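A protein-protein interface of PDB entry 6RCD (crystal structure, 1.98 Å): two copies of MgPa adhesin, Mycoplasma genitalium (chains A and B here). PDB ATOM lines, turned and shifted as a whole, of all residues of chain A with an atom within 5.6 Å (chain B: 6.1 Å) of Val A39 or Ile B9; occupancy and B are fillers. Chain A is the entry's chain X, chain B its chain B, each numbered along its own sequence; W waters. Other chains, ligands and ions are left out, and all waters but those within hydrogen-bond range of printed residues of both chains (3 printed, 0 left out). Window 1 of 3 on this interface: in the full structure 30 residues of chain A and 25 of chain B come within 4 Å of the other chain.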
ATOM      1  N   TYR A  34      11.401 -26.821  13.630  1.00  0.00           N
ATOM      2  CA  TYR A  34      12.395 -25.740  13.690  1.00  0.00           C
ATOM      3  C   TYR A  34      13.775 -26.116  13.128  1.00  0.00           C
ATOM      4  O   TYR A  34      14.605 -25.228  12.916  1.00  0.00           O
ATOM      5  CB  TYR A  34      12.531 -25.219  15.145  1.00  0.00           C
ATOM      6  CG  TYR A  34      11.217 -24.782  15.765  1.00  0.00           C
ATOM      7  CD1 TYR A  34      10.318 -23.986  15.058  1.00  0.00           C
ATOM      8  CD2 TYR A  34      10.890 -25.130  17.072  1.00  0.00           C
ATOM      9  CE1 TYR A  34       9.104 -23.589  15.623  1.00  0.00           C
ATOM     10  CE2 TYR A  34       9.687 -24.723  17.652  1.00  0.00           C
ATOM     11  CZ  TYR A  34       8.794 -23.965  16.921  1.00  0.00           C
ATOM     12  OH  TYR A  34       7.615 -23.573  17.506  1.00  0.00           O
ATOM     13  N   VAL A  35      14.048 -27.413  12.910  1.00  0.00           N
ATOM     14  CA  VAL A  35      15.382 -27.829  12.412  1.00  0.00           C
ATOM     15  C   VAL A  35      15.774 -27.060  11.112  1.00  0.00           C
ATOM     16  O   VAL A  35      16.869 -26.471  11.109  1.00  0.00           O
ATOM     17  CB  VAL A  35      15.528 -29.369  12.295  1.00  0.00           C
ATOM     18  CG1 VAL A  35      16.846 -29.766  11.616  1.00  0.00           C
ATOM     19  CG2 VAL A  35      15.418 -30.023  13.677  1.00  0.00           C
ATOM     20  N   PRO A  36      14.879 -26.922  10.080  1.00  0.00           N
ATOM     21  CA  PRO A  36      15.268 -26.162   8.869  1.00  0.00           C
ATOM     22  C   PRO A  36      15.461 -24.661   9.082  1.00  0.00           C
ATOM     23  O   PRO A  36      16.092 -24.013   8.242  1.00  0.00           O
ATOM     24  CB  PRO A  36      14.110 -26.430   7.892  1.00  0.00           C
ATOM     25  CG  PRO A  36      13.474 -27.692   8.385  1.00  0.00           C
ATOM     26  CD  PRO A  36      13.549 -27.543   9.888  1.00  0.00           C
ATOM     27  N   LEU A  37      14.956 -24.116  10.198  1.00  0.00           N
ATOM     28  CA  LEU A  37      15.160 -22.703  10.557  1.00  0.00           C
ATOM     29  C   LEU A  37      16.527 -22.492  11.149  1.00  0.00           C
ATOM     30  O   LEU A  37      17.081 -21.406  10.997  1.00  0.00           O
ATOM     31  CB  LEU A  37      14.147 -22.202  11.627  1.00  0.00           C
ATOM     32  CG  LEU A  37      12.694 -22.222  11.303  1.00  0.00           C
ATOM     33  CD1 LEU A  37      11.890 -21.549  12.446  1.00  0.00           C
ATOM     34  CD2 LEU A  37      12.431 -21.554   9.989  1.00  0.00           C
ATOM     35  N   LEU A  38      17.035 -23.484  11.917  1.00  0.00           N
ATOM     36  CA  LEU A  38      18.297 -23.330  12.632  1.00  0.00           C
ATOM     37  C   LEU A  38      19.490 -23.728  11.792  1.00  0.00           C
ATOM     38  O   LEU A  38      20.589 -23.217  12.009  1.00  0.00           O
ATOM     39  CB  LEU A  38      18.285 -24.139  13.949  1.00  0.00           C
ATOM     40  CG  LEU A  38      17.112 -23.934  14.943  1.00  0.00           C
ATOM     41  CD1 LEU A  38      17.406 -24.633  16.261  1.00  0.00           C
ATOM     42  CD2 LEU A  38      16.802 -22.455  15.189  1.00  0.00           C
ATOM     43  N   VAL A  39      19.285 -24.695  10.885  1.00  0.00           N
ATOM     44  CA  VAL A  39      20.331 -25.245  10.017  1.00  0.00           C
ATOM     45  C   VAL A  39      19.983 -24.962   8.573  1.00  0.00           C
ATOM     46  O   VAL A  39      18.847 -25.224   8.150  1.00  0.00           O
ATOM     47  CB  VAL A  39      20.536 -26.768  10.250  1.00  0.00           C
ATOM     48  CG1 VAL A  39      21.732 -27.302   9.450  1.00  0.00           C
ATOM     49  CG2 VAL A  39      20.705 -27.081  11.739  1.00  0.00           C
ATOM     50  N   ASN A  40      20.971 -24.459   7.809  1.00  0.00           N
ATOM     51  CA  ASN A  40      20.809 -24.227   6.392  1.00  0.00           C
ATOM     52  C   ASN A  40      20.979 -25.592   5.702  1.00  0.00           C
ATOM     53  O   ASN A  40      22.099 -26.034   5.464  1.00  0.00           O
ATOM     54  CB  ASN A  40      21.853 -23.200   5.890  1.00  0.00           C
ATOM     55  CG  ASN A  40      21.710 -22.872   4.438  1.00  0.00           C
ATOM     56  OD1 ASN A  40      20.635 -23.000   3.828  1.00  0.00           O
ATOM     57  ND2 ASN A  40      22.797 -22.434   3.851  1.00  0.00           N
ATOM     58  N   LEU A  41      19.867 -26.254   5.391  1.00  0.00           N
ATOM     59  CA  LEU A  41      19.885 -27.576   4.764  1.00  0.00           C
ATOM     60  C   LEU A  41      20.089 -27.508   3.269  1.00  0.00           C
ATOM     61  O   LEU A  41      19.567 -26.585   2.658  1.00  0.00           O
ATOM     62  CB  LEU A  41      18.588 -28.324   5.059  1.00  0.00           C
ATOM     63  CG  LEU A  41      18.263 -28.547   6.543  1.00  0.00           C
ATOM     64  CD1 LEU A  41      16.864 -29.110   6.694  1.00  0.00           C
ATOM     65  CD2 LEU A  41      19.295 -29.435   7.234  1.00  0.00           C
ATOM     66  N   ILE A  50      17.616 -36.454  10.180  1.00  0.00           N
ATOM     67  CA  ILE A  50      18.494 -35.835  11.180  1.00  0.00           C
ATOM     68  C   ILE A  50      17.715 -35.333  12.407  1.00  0.00           C
ATOM     69  O   ILE A  50      16.497 -35.162  12.367  1.00  0.00           O
ATOM     70  CB  ILE A  50      19.359 -34.679  10.565  1.00  0.00           C
ATOM     71  CG1 ILE A  50      18.454 -33.515  10.041  1.00  0.00           C
ATOM     72  CG2 ILE A  50      20.360 -35.188   9.503  1.00  0.00           C
ATOM     73  CD1 ILE A  50      19.151 -32.176   9.779  1.00  0.00           C
ATOM     74  N   LEU A  52      18.621 -32.547  16.101  1.00  0.00           N
ATOM     75  CA  LEU A  52      19.546 -31.666  16.799  1.00  0.00           C
ATOM     76  C   LEU A  52      19.377 -31.821  18.271  1.00  0.00           C
ATOM     77  O   LEU A  52      18.316 -31.502  18.813  1.00  0.00           O
ATOM     78  CB  LEU A  52      19.308 -30.188  16.438  1.00  0.00           C
ATOM     79  CG  LEU A  52      19.620 -29.702  15.044  1.00  0.00           C
ATOM     80  CD1 LEU A  52      19.228 -28.196  14.924  1.00  0.00           C
ATOM     81  CD2 LEU A  52      21.121 -29.923  14.691  1.00  0.00           C
ATOM     82  N   THR A  91      28.287 -26.756  18.010  1.00  0.00           N
ATOM     83  CA  THR A  91      28.118 -25.323  17.755  1.00  0.00           C
ATOM     84  C   THR A  91      27.272 -24.600  18.799  1.00  0.00           C
ATOM     85  O   THR A  91      26.289 -25.140  19.299  1.00  0.00           O
ATOM     86  CB  THR A  91      27.572 -25.064  16.306  1.00  0.00           C
ATOM     87  OG1 THR A  91      27.428 -23.655  16.098  1.00  0.00           O
ATOM     88  CG2 THR A  91      26.216 -25.682  16.065  1.00  0.00           C
ATOM     89  N   PHE A  93      25.330 -20.911  19.068  1.00  0.00           N
ATOM     90  CA  PHE A  93      24.906 -19.803  18.210  1.00  0.00           C
ATOM     91  C   PHE A  93      23.629 -19.165  18.724  1.00  0.00           C
ATOM     92  O   PHE A  93      22.902 -19.753  19.542  1.00  0.00           O
ATOM     93  CB  PHE A  93      24.722 -20.312  16.746  1.00  0.00           C
ATOM     94  CG  PHE A  93      23.522 -21.213  16.523  1.00  0.00           C
ATOM     95  CD1 PHE A  93      23.457 -22.479  17.101  1.00  0.00           C
ATOM     96  CD2 PHE A  93      22.445 -20.787  15.757  1.00  0.00           C
ATOM     97  CE1 PHE A  93      22.326 -23.293  16.927  1.00  0.00           C
ATOM     98  CE2 PHE A  93      21.333 -21.616  15.556  1.00  0.00           C
ATOM     99  CZ  PHE A  93      21.281 -22.860  16.146  1.00  0.00           C
ATOM    100  N   ASN B   7      22.073 -16.145  13.652  1.00  0.00           N
ATOM    101  CA  ASN B   7      22.712 -16.974  12.638  1.00  0.00           C
ATOM    102  C   ASN B   7      21.933 -18.233  12.387  1.00  0.00           C
ATOM    103  O   ASN B   7      21.378 -18.817  13.322  1.00  0.00           O
ATOM    104  CB  ASN B   7      24.111 -17.440  13.116  1.00  0.00           C
ATOM    105  CG  ASN B   7      25.255 -16.519  12.845  1.00  0.00           C
ATOM    106  OD1 ASN B   7      25.816 -15.945  13.760  1.00  0.00           O
ATOM    107  ND2 ASN B   7      25.664 -16.405  11.595  1.00  0.00           N
ATOM    108  N   GLN B   8      22.006 -18.727  11.136  1.00  0.00           N
ATOM    109  CA  GLN B   8      21.509 -20.048  10.726  1.00  0.00           C
ATOM    110  C   GLN B   8      22.831 -20.828  10.550  1.00  0.00           C
ATOM    111  O   GLN B   8      23.776 -20.256  10.026  1.00  0.00           O
ATOM    112  CB  GLN B   8      20.758 -19.936   9.385  1.00  0.00           C
ATOM    113  CG  GLN B   8      19.878 -21.149   9.070  1.00  0.00           C
ATOM    114  CD  GLN B   8      19.308 -21.124   7.663  1.00  0.00           C
ATOM    115  OE1 GLN B   8      19.966 -20.702   6.704  1.00  0.00           O
ATOM    116  NE2 GLN B   8      18.082 -21.618   7.500  1.00  0.00           N
ATOM    117  N   ILE B   9      22.929 -22.079  10.989  1.00  0.00           N
ATOM    118  CA  ILE B   9      24.194 -22.825  10.876  1.00  0.00           C
ATOM    119  C   ILE B   9      24.336 -23.517   9.543  1.00  0.00           C
ATOM    120  O   ILE B   9      23.401 -24.189   9.132  1.00  0.00           O
ATOM    121  CB  ILE B   9      24.366 -23.821  12.066  1.00  0.00           C
ATOM    122  CG1 ILE B   9      24.310 -23.098  13.425  1.00  0.00           C
ATOM    123  CG2 ILE B   9      25.655 -24.656  11.953  1.00  0.00           C
ATOM    124  CD1 ILE B   9      25.394 -21.999  13.620  1.00  0.00           C
ATOM    125  N   ASP B  10      25.519 -23.412   8.889  1.00  0.00           N
ATOM    126  CA  ASP B  10      25.729 -24.153   7.644  1.00  0.00           C
ATOM    127  C   ASP B  10      25.813 -25.639   7.969  1.00  0.00           C
ATOM    128  O   ASP B  10      26.474 -26.043   8.932  1.00  0.00           O
ATOM    129  CB  ASP B  10      26.996 -23.699   6.913  1.00  0.00           C
ATOM    130  CG  ASP B  10      26.867 -22.324   6.284  1.00  0.00           C
ATOM    131  OD1 ASP B  10      25.760 -21.997   5.777  1.00  0.00           O
ATOM    132  OD2 ASP B  10      27.865 -21.579   6.289  1.00  0.00           O
ATOM    133  N   PHE B  11      25.089 -26.437   7.202  1.00  0.00           N
ATOM    134  CA  PHE B  11      25.007 -27.888   7.354  1.00  0.00           C
ATOM    135  C   PHE B  11      26.381 -28.576   7.443  1.00  0.00           C
ATOM    136  O   PHE B  11      26.542 -29.458   8.275  1.00  0.00           O
ATOM    137  CB  PHE B  11      24.169 -28.464   6.205  1.00  0.00           C
ATOM    138  CG  PHE B  11      23.741 -29.881   6.437  1.00  0.00           C
ATOM    139  CD1 PHE B  11      22.758 -30.183   7.375  1.00  0.00           C
ATOM    140  CD2 PHE B  11      24.328 -30.924   5.728  1.00  0.00           C
ATOM    141  CE1 PHE B  11      22.334 -31.485   7.575  1.00  0.00           C
ATOM    142  CE2 PHE B  11      23.921 -32.239   5.950  1.00  0.00           C
ATOM    143  CZ  PHE B  11      22.922 -32.506   6.870  1.00  0.00           C
ATOM    144  N   ARG B  13      29.044 -27.583   8.835  1.00  0.00           N
ATOM    145  CA  ARG B  13      29.658 -27.374  10.150  1.00  0.00           C
ATOM    146  C   ARG B  13      29.203 -28.453  11.144  1.00  0.00           C
ATOM    147  O   ARG B  13      29.829 -28.632  12.180  1.00  0.00           O
ATOM    148  CB  ARG B  13      29.308 -25.978  10.698  1.00  0.00           C
ATOM    149  CG  ARG B  13      29.902 -24.825   9.872  1.00  0.00           C
ATOM    150  CD  ARG B  13      31.400 -24.691  10.055  1.00  0.00           C
ATOM    151  NE  ARG B  13      31.926 -23.602   9.238  1.00  0.00           N
ATOM    152  CZ  ARG B  13      33.197 -23.220   9.220  1.00  0.00           C
ATOM    153  NH1 ARG B  13      34.090 -23.824   9.995  1.00  0.00           N
ATOM    154  NH2 ARG B  13      33.584 -22.230   8.430  1.00  0.00           N
ATOM    155  N   LEU B  14      28.098 -29.139  10.840  1.00  0.00           N
ATOM    156  CA  LEU B  14      27.491 -30.129  11.735  1.00  0.00           C
ATOM    157  C   LEU B  14      27.538 -31.557  11.232  1.00  0.00           C
ATOM    158  O   LEU B  14      27.495 -32.477  12.053  1.00  0.00           O
ATOM    159  CB  LEU B  14      26.007 -29.769  11.959  1.00  0.00           C
ATOM    160  CG  LEU B  14      25.700 -28.439  12.623  1.00  0.00           C
ATOM    161  CD1 LEU B  14      24.233 -28.143  12.540  1.00  0.00           C
ATOM    162  CD2 LEU B  14      26.126 -28.471  14.075  1.00  0.00           C
HETATM  163  O   HOH W   1      17.856 -22.643   4.364  1.00  0.00           O
HETATM  164  O   HOH W   2      24.912 -24.603   4.323  1.00  0.00           O
HETATM  165  O   HOH W   3      18.574 -19.558  13.176  1.00  0.00           O
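The backbone carbonyl oxygen (O) of Pro A36 is in hydrogen-bond range of the side-chain amide nitrogen (NE2) of Gln B8, at 3.2 Å.
The backbone NH (N) of Ile B9 sits at hydrogen-bond distance from the backbone carbonyl oxygen (O) of Leu A38 (2.8 Å).
The backbone carbonyl oxygen of Ile B9 is in hydrogen-bond range of the backbone NH of Asn A40 (2.8 Å).
O of Asn A40 sits close to N of Phe B11 (3.5 Å).
Among the printed residues, merely in contact across the chains: Asn A40 with Gln B8 (3.2 Å), Phe A93 with Asn B7 (3.3 Å), Val A39 with Ile B9 (3.4 Å), Leu A37 with Gln B8 (3.4 Å), Thr A91 with Leu B14 (3.4 Å), Leu A38 with Gln B8 (3.5 Å), Phe A93 with Ile B9 (3.5 Å), Leu A41 with Phe B11 (3.5 Å), Asn A40 with Asp B10 (3.6 Å), Thr A91 with Ile B9 (3.6 Å), Val A39 with Phe B11 (3.7 Å), Val A39 with Gln B8 (3.7 Å), Val A39 with Leu B14 (3.8 Å) and Ile A50 with Phe B11 (3.9 Å).
Ile B9 touches five residues of chain A.
Printed residues of chain A within 4 Å of Asn B7: Phe A93.
Of the printed residues of chain B, Leu A38 touches Gln B8 and Ile B9.
Arg B13 touches none of the printed residues of chain A.
The nearest residue of chain B that does not touch Val A39 is Asp B10 (4.6 Å).
Of the 12 printed residues of chain A, 9 touch a printed residue of chain B.
Hydrophobic or aromatic side chains of chain A within 4 Å of the printed part of chain B: Val A39, Leu A41, Ile A50 and Phe A93.
Of the 7 printed residues of chain B, 6 touch a printed residue of chain A.
Printed residues of chain B that touch a printed residue of chain A: Asn B7, Gln B8, Ile B9, Asp B10, Phe B11 and Leu B14.
Among the printed residues, 18 pairs touch across the chains.
Among the printed residues, no Asp or Glu carboxylate lies within 4 Å of a Lys or Arg side-chain nitrogen of the other chain.
No position is printed for both chains.
Water W1 bridges the side-chain amide oxygen (OD1) of Asn A40 and the side-chain amide nitrogen (NE2) of Gln B8.
Water W3 lies within hydrogen-bond range of the backbone carbonyl oxygen (O) of Asn B7 (2.9 Å) and the backbone carbonyl oxygen (O) of Leu A37 (3.2 Å).
Water W2 lies within hydrogen-bond range of ND2 of Asn A40 (3.1 Å), OD1 of Asp B10 (3.1 Å) and N of Phe B11 (3.4 Å).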
